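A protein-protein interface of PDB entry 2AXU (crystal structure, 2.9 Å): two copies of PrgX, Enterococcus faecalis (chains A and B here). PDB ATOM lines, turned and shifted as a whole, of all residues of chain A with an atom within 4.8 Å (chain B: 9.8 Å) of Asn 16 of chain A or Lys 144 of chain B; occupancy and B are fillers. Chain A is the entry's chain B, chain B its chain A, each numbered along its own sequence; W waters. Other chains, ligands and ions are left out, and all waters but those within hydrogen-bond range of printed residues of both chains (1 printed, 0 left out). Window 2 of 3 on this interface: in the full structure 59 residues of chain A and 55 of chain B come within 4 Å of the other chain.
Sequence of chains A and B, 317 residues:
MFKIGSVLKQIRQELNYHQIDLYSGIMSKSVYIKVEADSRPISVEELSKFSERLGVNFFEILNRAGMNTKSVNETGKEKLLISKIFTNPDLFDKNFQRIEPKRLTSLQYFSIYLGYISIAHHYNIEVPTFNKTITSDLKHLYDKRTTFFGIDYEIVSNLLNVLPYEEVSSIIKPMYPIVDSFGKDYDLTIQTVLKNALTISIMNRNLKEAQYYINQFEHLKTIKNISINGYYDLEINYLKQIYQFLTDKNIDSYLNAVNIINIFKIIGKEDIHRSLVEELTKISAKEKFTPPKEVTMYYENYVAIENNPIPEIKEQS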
ATOM      1  N   ARG A  12      -2.057 -12.449  -2.474  1.00  0.00           N
ATOM      2  CA  ARG A  12      -3.008 -13.552  -2.406  1.00  0.00           C
ATOM      3  C   ARG A  12      -3.485 -13.958  -3.787  1.00  0.00           C
ATOM      4  O   ARG A  12      -3.507 -15.142  -4.119  1.00  0.00           O
ATOM      5  CB  ARG A  12      -4.219 -13.181  -1.549  1.00  0.00           C
ATOM      6  CG  ARG A  12      -5.210 -14.326  -1.389  1.00  0.00           C
ATOM      7  CD  ARG A  12      -6.317 -13.983  -0.409  1.00  0.00           C
ATOM      8  NE  ARG A  12      -7.171 -12.904  -0.894  1.00  0.00           N
ATOM      9  CZ  ARG A  12      -7.961 -12.997  -1.961  1.00  0.00           C
ATOM     10  NH1 ARG A  12      -8.012 -14.123  -2.665  1.00  0.00           N
ATOM     11  NH2 ARG A  12      -8.704 -11.960  -2.327  1.00  0.00           N
ATOM     12  N   GLN A  13      -3.861 -12.971  -4.592  1.00  0.00           N
ATOM     13  CA  GLN A  13      -4.347 -13.244  -5.936  1.00  0.00           C
ATOM     14  C   GLN A  13      -3.215 -13.700  -6.854  1.00  0.00           C
ATOM     15  O   GLN A  13      -3.381 -14.636  -7.634  1.00  0.00           O
ATOM     16  CB  GLN A  13      -5.040 -12.001  -6.493  1.00  0.00           C
ATOM     17  CG  GLN A  13      -6.116 -11.463  -5.542  1.00  0.00           C
ATOM     18  CD  GLN A  13      -6.915 -10.308  -6.116  1.00  0.00           C
ATOM     19  OE1 GLN A  13      -6.362  -9.276  -6.502  1.00  0.00           O
ATOM     20  NE2 GLN A  13      -8.230 -10.474  -6.159  1.00  0.00           N
ATOM     21  N   GLU A  14      -2.061 -13.046  -6.752  1.00  0.00           N
ATOM     22  CA  GLU A  14      -0.902 -13.413  -7.567  1.00  0.00           C
ATOM     23  C   GLU A  14      -0.654 -14.915  -7.462  1.00  0.00           C
ATOM     24  O   GLU A  14      -0.489 -15.606  -8.469  1.00  0.00           O
ATOM     25  CB  GLU A  14       0.342 -12.661  -7.081  1.00  0.00           C
ATOM     26  CG  GLU A  14       1.653 -13.050  -7.768  1.00  0.00           C
ATOM     27  CD  GLU A  14       1.652 -12.742  -9.249  1.00  0.00           C
ATOM     28  OE1 GLU A  14       1.106 -11.687  -9.630  1.00  0.00           O
ATOM     29  OE2 GLU A  14       2.204 -13.543 -10.030  1.00  0.00           O
ATOM     30  N   LEU A  15      -0.628 -15.410  -6.229  1.00  0.00           N
ATOM     31  CA  LEU A  15      -0.388 -16.822  -5.978  1.00  0.00           C
ATOM     32  C   LEU A  15      -1.641 -17.648  -6.202  1.00  0.00           C
ATOM     33  O   LEU A  15      -1.678 -18.836  -5.891  1.00  0.00           O
ATOM     34  CB  LEU A  15       0.141 -17.025  -4.553  1.00  0.00           C
ATOM     35  CG  LEU A  15       1.456 -16.285  -4.262  1.00  0.00           C
ATOM     36  CD1 LEU A  15       1.909 -16.584  -2.842  1.00  0.00           C
ATOM     37  CD2 LEU A  15       2.529 -16.701  -5.264  1.00  0.00           C
ATOM     38  N   ASN A  16      -2.669 -17.007  -6.745  1.00  0.00           N
ATOM     39  CA  ASN A  16      -3.928 -17.678  -7.036  1.00  0.00           C
ATOM     40  C   ASN A  16      -4.546 -18.360  -5.815  1.00  0.00           C
ATOM     41  O   ASN A  16      -4.749 -19.573  -5.803  1.00  0.00           O
ATOM     42  CB  ASN A  16      -3.718 -18.715  -8.139  1.00  0.00           C
ATOM     43  CG  ASN A  16      -5.017 -19.195  -8.741  1.00  0.00           C
ATOM     44  OD1 ASN A  16      -5.069 -20.256  -9.362  1.00  0.00           O
ATOM     45  ND2 ASN A  16      -6.076 -18.409  -8.575  1.00  0.00           N
ATOM     46  N   TYR A  17      -4.836 -17.573  -4.787  1.00  0.00           N
ATOM     47  CA  TYR A  17      -5.447 -18.088  -3.568  1.00  0.00           C
ATOM     48  C   TYR A  17      -6.790 -17.396  -3.388  1.00  0.00           C
ATOM     49  O   TYR A  17      -6.969 -16.264  -3.830  1.00  0.00           O
ATOM     50  CB  TYR A  17      -4.575 -17.779  -2.342  1.00  0.00           C
ATOM     51  CG  TYR A  17      -3.331 -18.624  -2.162  1.00  0.00           C
ATOM     52  CD1 TYR A  17      -3.403 -20.016  -2.102  1.00  0.00           C
ATOM     53  CD2 TYR A  17      -2.089 -18.023  -1.965  1.00  0.00           C
ATOM     54  CE1 TYR A  17      -2.267 -20.788  -1.842  1.00  0.00           C
ATOM     55  CE2 TYR A  17      -0.946 -18.784  -1.704  1.00  0.00           C
ATOM     56  CZ  TYR A  17      -1.043 -20.163  -1.642  1.00  0.00           C
ATOM     57  OH  TYR A  17       0.078 -20.915  -1.371  1.00  0.00           O
ATOM     58  N   HIS A  18      -7.731 -18.074  -2.740  1.00  0.00           N
ATOM     59  CA  HIS A  18      -9.042 -17.489  -2.483  1.00  0.00           C
ATOM     60  C   HIS A  18      -8.958 -16.875  -1.100  1.00  0.00           C
ATOM     61  O   HIS A  18      -7.993 -17.118  -0.372  1.00  0.00           O
ATOM     62  CB  HIS A  18     -10.141 -18.556  -2.505  1.00  0.00           C
ATOM     63  CG  HIS A  18     -10.196 -19.338  -3.778  1.00  0.00           C
ATOM     64  ND1 HIS A  18     -10.329 -18.742  -5.014  1.00  0.00           N
ATOM     65  CD2 HIS A  18     -10.128 -20.671  -4.007  1.00  0.00           C
ATOM     66  CE1 HIS A  18     -10.340 -19.675  -5.950  1.00  0.00           C
ATOM     67  NE2 HIS A  18     -10.220 -20.854  -5.365  1.00  0.00           N
ATOM     68  N   LEU B 104       3.403 -28.524  -2.424  1.00  0.00           N
ATOM     69  CA  LEU B 104       2.744 -27.447  -3.160  1.00  0.00           C
ATOM     70  C   LEU B 104       1.874 -26.566  -2.271  1.00  0.00           C
ATOM     71  O   LEU B 104       1.339 -25.558  -2.732  1.00  0.00           O
ATOM     72  CB  LEU B 104       1.877 -28.012  -4.288  1.00  0.00           C
ATOM     73  CG  LEU B 104       2.514 -28.860  -5.393  1.00  0.00           C
ATOM     74  CD1 LEU B 104       1.448 -29.237  -6.417  1.00  0.00           C
ATOM     75  CD2 LEU B 104       3.633 -28.089  -6.067  1.00  0.00           C
ATOM     76  N   THR B 105       1.730 -26.948  -1.005  1.00  0.00           N
ATOM     77  CA  THR B 105       0.913 -26.198  -0.054  1.00  0.00           C
ATOM     78  C   THR B 105       1.199 -24.695  -0.141  1.00  0.00           C
ATOM     79  O   THR B 105       0.276 -23.883  -0.249  1.00  0.00           O
ATOM     80  CB  THR B 105       1.166 -26.689   1.381  1.00  0.00           C
ATOM     81  OG1 THR B 105       1.213 -28.121   1.387  1.00  0.00           O
ATOM     82  CG2 THR B 105       0.045 -26.240   2.305  1.00  0.00           C
ATOM     83  N   LEU B 107       4.670 -21.811  -1.410  1.00  0.00           N
ATOM     84  CA  LEU B 107       5.965 -21.724  -2.065  1.00  0.00           C
ATOM     85  C   LEU B 107       7.089 -22.055  -1.083  1.00  0.00           C
ATOM     86  O   LEU B 107       8.186 -22.443  -1.498  1.00  0.00           O
ATOM     87  CB  LEU B 107       6.164 -20.324  -2.650  1.00  0.00           C
ATOM     88  CG  LEU B 107       5.310 -20.004  -3.876  1.00  0.00           C
ATOM     89  CD1 LEU B 107       5.442 -18.535  -4.254  1.00  0.00           C
ATOM     90  CD2 LEU B 107       5.749 -20.893  -5.021  1.00  0.00           C
ATOM     91  N   ASP B 137       4.859 -29.861 -11.741  1.00  0.00           N
ATOM     92  CA  ASP B 137       4.902 -28.953 -10.592  1.00  0.00           C
ATOM     93  C   ASP B 137       5.252 -27.516 -10.954  1.00  0.00           C
ATOM     94  O   ASP B 137       4.479 -26.595 -10.694  1.00  0.00           O
ATOM     95  CB  ASP B 137       5.927 -29.450  -9.569  1.00  0.00           C
ATOM     96  CG  ASP B 137       5.405 -30.581  -8.719  1.00  0.00           C
ATOM     97  OD1 ASP B 137       6.203 -31.151  -7.943  1.00  0.00           O
ATOM     98  OD2 ASP B 137       4.203 -30.895  -8.818  1.00  0.00           O
ATOM     99  N   LEU B 138       6.429 -27.333 -11.542  1.00  0.00           N
ATOM    100  CA  LEU B 138       6.894 -26.006 -11.925  1.00  0.00           C
ATOM    101  C   LEU B 138       5.904 -25.269 -12.819  1.00  0.00           C
ATOM    102  O   LEU B 138       5.744 -24.053 -12.693  1.00  0.00           O
ATOM    103  CB  LEU B 138       8.255 -26.104 -12.615  1.00  0.00           C
ATOM    104  CG  LEU B 138       9.373 -26.650 -11.725  1.00  0.00           C
ATOM    105  CD1 LEU B 138      10.655 -26.798 -12.528  1.00  0.00           C
ATOM    106  CD2 LEU B 138       9.588 -25.717 -10.543  1.00  0.00           C
ATOM    107  N   LYS B 139       5.242 -25.991 -13.722  1.00  0.00           N
ATOM    108  CA  LYS B 139       4.260 -25.364 -14.599  1.00  0.00           C
ATOM    109  C   LYS B 139       3.089 -24.864 -13.769  1.00  0.00           C
ATOM    110  O   LYS B 139       2.575 -23.768 -13.995  1.00  0.00           O
ATOM    111  CB  LYS B 139       3.762 -26.351 -15.656  1.00  0.00           C
ATOM    112  CG  LYS B 139       4.638 -26.401 -16.894  1.00  0.00           C
ATOM    113  CD  LYS B 139       3.997 -27.223 -17.993  1.00  0.00           C
ATOM    114  CE  LYS B 139       4.731 -27.035 -19.309  1.00  0.00           C
ATOM    115  NZ  LYS B 139       6.176 -27.370 -19.191  1.00  0.00           N
ATOM    116  N   HIS B 140       2.681 -25.677 -12.800  1.00  0.00           N
ATOM    117  CA  HIS B 140       1.576 -25.342 -11.910  1.00  0.00           C
ATOM    118  C   HIS B 140       1.905 -24.109 -11.078  1.00  0.00           C
ATOM    119  O   HIS B 140       1.022 -23.314 -10.750  1.00  0.00           O
ATOM    120  CB  HIS B 140       1.291 -26.530 -10.988  1.00  0.00           C
ATOM    121  CG  HIS B 140       0.282 -26.244  -9.921  1.00  0.00           C
ATOM    122  ND1 HIS B 140       0.542 -25.413  -8.852  1.00  0.00           N
ATOM    123  CD2 HIS B 140      -0.990 -26.679  -9.758  1.00  0.00           C
ATOM    124  CE1 HIS B 140      -0.524 -25.349  -8.076  1.00  0.00           C
ATOM    125  NE2 HIS B 140      -1.468 -26.108  -8.603  1.00  0.00           N
ATOM    126  N   LEU B 141       3.184 -23.946 -10.750  1.00  0.00           N
ATOM    127  CA  LEU B 141       3.633 -22.827  -9.937  1.00  0.00           C
ATOM    128  C   LEU B 141       4.018 -21.549 -10.671  1.00  0.00           C
ATOM    129  O   LEU B 141       4.052 -20.485 -10.055  1.00  0.00           O
ATOM    130  CB  LEU B 141       4.829 -23.251  -9.087  1.00  0.00           C
ATOM    131  CG  LEU B 141       4.623 -24.170  -7.887  1.00  0.00           C
ATOM    132  CD1 LEU B 141       5.990 -24.559  -7.309  1.00  0.00           C
ATOM    133  CD2 LEU B 141       3.762 -23.464  -6.845  1.00  0.00           C
ATOM    134  N   TYR B 142       4.301 -21.626 -11.968  1.00  0.00           N
ATOM    135  CA  TYR B 142       4.734 -20.421 -12.667  1.00  0.00           C
ATOM    136  C   TYR B 142       4.065 -19.962 -13.960  1.00  0.00           C
ATOM    137  O   TYR B 142       4.413 -18.902 -14.485  1.00  0.00           O
ATOM    138  CB  TYR B 142       6.243 -20.503 -12.889  1.00  0.00           C
ATOM    139  CG  TYR B 142       7.011 -20.427 -11.594  1.00  0.00           C
ATOM    140  CD1 TYR B 142       7.065 -19.236 -10.869  1.00  0.00           C
ATOM    141  CD2 TYR B 142       7.646 -21.550 -11.066  1.00  0.00           C
ATOM    142  CE1 TYR B 142       7.727 -19.167  -9.654  1.00  0.00           C
ATOM    143  CE2 TYR B 142       8.311 -21.492  -9.848  1.00  0.00           C
ATOM    144  CZ  TYR B 142       8.347 -20.297  -9.148  1.00  0.00           C
ATOM    145  OH  TYR B 142       8.995 -20.229  -7.939  1.00  0.00           O
ATOM    146  N   ASP B 143       3.104 -20.720 -14.477  1.00  0.00           N
ATOM    147  CA  ASP B 143       2.452 -20.301 -15.713  1.00  0.00           C
ATOM    148  C   ASP B 143       1.545 -19.077 -15.579  1.00  0.00           C
ATOM    149  O   ASP B 143       1.437 -18.282 -16.513  1.00  0.00           O
ATOM    150  CB  ASP B 143       1.671 -21.464 -16.328  1.00  0.00           C
ATOM    151  CG  ASP B 143       2.522 -22.294 -17.272  1.00  0.00           C
ATOM    152  OD1 ASP B 143       1.968 -23.186 -17.949  1.00  0.00           O
ATOM    153  OD2 ASP B 143       3.746 -22.053 -17.340  1.00  0.00           O
ATOM    154  N   LYS B 144       0.905 -18.914 -14.425  1.00  0.00           N
ATOM    155  CA  LYS B 144       0.011 -17.778 -14.208  1.00  0.00           C
ATOM    156  C   LYS B 144       0.672 -16.659 -13.404  1.00  0.00           C
ATOM    157  O   LYS B 144      -0.028 -15.884 -12.752  1.00  0.00           O
ATOM    158  CB  LYS B 144      -1.240 -18.213 -13.443  1.00  0.00           C
ATOM    159  CG  LYS B 144      -2.028 -19.359 -14.041  1.00  0.00           C
ATOM    160  CD  LYS B 144      -3.231 -19.658 -13.154  1.00  0.00           C
ATOM    161  CE  LYS B 144      -4.061 -20.819 -13.675  1.00  0.00           C
ATOM    162  NZ  LYS B 144      -5.264 -21.060 -12.826  1.00  0.00           N
ATOM    163  N   ARG B 145       1.996 -16.556 -13.448  1.00  0.00           N
ATOM    164  CA  ARG B 145       2.687 -15.533 -12.659  1.00  0.00           C
ATOM    165  C   ARG B 145       3.033 -14.254 -13.405  1.00  0.00           C
ATOM    166  O   ARG B 145       3.235 -14.269 -14.615  1.00  0.00           O
ATOM    167  CB  ARG B 145       3.963 -16.125 -12.047  1.00  0.00           C
ATOM    168  CG  ARG B 145       3.714 -17.267 -11.064  1.00  0.00           C
ATOM    169  CD  ARG B 145       2.942 -16.795  -9.833  1.00  0.00           C
ATOM    170  NE  ARG B 145       3.706 -15.825  -9.047  1.00  0.00           N
ATOM    171  CZ  ARG B 145       4.666 -16.140  -8.182  1.00  0.00           C
ATOM    172  NH1 ARG B 145       4.987 -17.408  -7.970  1.00  0.00           N
ATOM    173  NH2 ARG B 145       5.324 -15.183  -7.546  1.00  0.00           N
ATOM    174  N   THR B 146       3.103 -13.148 -12.664  1.00  0.00           N
ATOM    175  CA  THR B 146       3.437 -11.838 -13.229  1.00  0.00           C
ATOM    176  C   THR B 146       4.480 -11.130 -12.364  1.00  0.00           C
ATOM    177  O   THR B 146       5.351 -10.438 -12.882  1.00  0.00           O
ATOM    178  CB  THR B 146       2.198 -10.920 -13.345  1.00  0.00           C
ATOM    179  OG1 THR B 146       1.595 -10.766 -12.058  1.00  0.00           O
ATOM    180  CG2 THR B 146       1.174 -11.505 -14.302  1.00  0.00           C
ATOM    181  N   THR B 147       4.384 -11.292 -11.046  1.00  0.00           N
ATOM    182  CA  THR B 147       5.355 -10.692 -10.131  1.00  0.00           C
ATOM    183  C   THR B 147       6.022 -11.800  -9.320  1.00  0.00           C
ATOM    184  O   THR B 147       5.375 -12.781  -8.945  1.00  0.00           O
ATOM    185  CB  THR B 147       4.697  -9.670  -9.179  1.00  0.00           C
ATOM    186  OG1 THR B 147       3.552 -10.259  -8.560  1.00  0.00           O
ATOM    187  CG2 THR B 147       4.270  -8.434  -9.947  1.00  0.00           C
ATOM    188  N   PHE B 148       7.316 -11.644  -9.054  1.00  0.00           N
ATOM    189  CA  PHE B 148       8.056 -12.657  -8.312  1.00  0.00           C
ATOM    190  C   PHE B 148       8.571 -12.180  -6.969  1.00  0.00           C
ATOM    191  O   PHE B 148       9.135 -11.090  -6.861  1.00  0.00           O
ATOM    192  CB  PHE B 148       9.217 -13.165  -9.158  1.00  0.00           C
ATOM    193  CG  PHE B 148       8.785 -13.750 -10.458  1.00  0.00           C
ATOM    194  CD1 PHE B 148       8.737 -12.964 -11.604  1.00  0.00           C
ATOM    195  CD2 PHE B 148       8.346 -15.071 -10.523  1.00  0.00           C
ATOM    196  CE1 PHE B 148       8.253 -13.477 -12.800  1.00  0.00           C
ATOM    197  CE2 PHE B 148       7.859 -15.600 -11.716  1.00  0.00           C
ATOM    198  CZ  PHE B 148       7.810 -14.801 -12.858  1.00  0.00           C
ATOM    199  N   PHE B 149       8.387 -13.009  -5.946  1.00  0.00           N
ATOM    200  CA  PHE B 149       8.821 -12.663  -4.603  1.00  0.00           C
ATOM    201  C   PHE B 149      10.132 -13.321  -4.222  1.00  0.00           C
ATOM    202  O   PHE B 149      10.626 -14.209  -4.920  1.00  0.00           O
ATOM    203  CB  PHE B 149       7.744 -13.034  -3.591  1.00  0.00           C
ATOM    204  CG  PHE B 149       6.370 -12.628  -4.014  1.00  0.00           C
ATOM    205  CD1 PHE B 149       5.525 -13.541  -4.641  1.00  0.00           C
ATOM    206  CD2 PHE B 149       5.926 -11.323  -3.815  1.00  0.00           C
ATOM    207  CE1 PHE B 149       4.253 -13.155  -5.065  1.00  0.00           C
ATOM    208  CE2 PHE B 149       4.664 -10.928  -4.232  1.00  0.00           C
ATOM    209  CZ  PHE B 149       3.821 -11.843  -4.859  1.00  0.00           C
HETATM  210  O   HOH W   1       3.043 -19.806  -1.960  1.00  0.00           O
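OE1 of Glu 14 of chain A lies within hydrogen-bond range of OG1 of Thr 147 of chain B (3.0 Å). OG1 of Thr 146 of chain B lies within hydrogen-bond range of OE1 of Glu 14 of chain A (2.6 Å). The backbone carbonyl oxygen (O) of Thr 105 of chain B lies within hydrogen-bond range of the side-chain hydroxyl (OH) of Tyr 17 of chain A, at 3.2 Å. The side-chain carboxylate of Glu 14 of chain A lies within salt-bridge range of the guanidinium group of Arg 145 of chain B, 2.9 Å away.
The guanidinium group (NH1) of Arg 12 of chain A sits at hydrogen-bond distance from the backbone carbonyl oxygen (O) of Tyr 17 of chain A (2.7 Å). The backbone carbonyl oxygen of Thr 147 of chain B sits at hydrogen-bond distance from the guanidinium group of Arg 145 of chain B.
Among the printed residues, pairs that only touch across the chains: Glu 14 of chain A with Phe 149 of chain B, Leu 15 of chain A with Leu 107 of chain B, Leu 15 of chain A with Arg 145 of chain B, Leu 15 of chain A with Phe 149 of chain B and Asn 16 of chain A with Lys 144 of chain B.
Asn 16 of chain A touches one residue of chain B. Printed residues of chain A within 4 Å of Lys 144 of chain B: Asn 16 (3.6 Å). Of the printed residues of chain A, Thr 147 of chain B touches Glu 14 (3.0 Å). Of the printed residues of chain B, Glu 14 of chain A touches Arg 145 (2.9 Å), Thr 146 (2.6 Å), Thr 147 (3.0 Å) and Phe 149 (3.8 Å). Printed residues of chain A within 4 Å of Thr 146 of chain B: Glu 14 (2.6 Å). His 140 of chain B touches none of the printed residues of chain A. Leu 104 of chain B touches none of the printed residues of chain A. The nearest printed residue of chain B that does not touch Glu 14 of chain A is Lys 144 of chain B (4.2 Å).
Of the 7 printed residues of chain A, 4 touch a printed residue of chain B. Printed residues of chain A that touch a printed residue of chain B: Glu 14, Leu 15, Asn 16 and Tyr 17.
No position is printed for both chains.
Water W1 lies within hydrogen-bond range of the backbone NH of Leu 107 of chain B and the side-chain hydroxyl of Tyr 17 of chain A.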
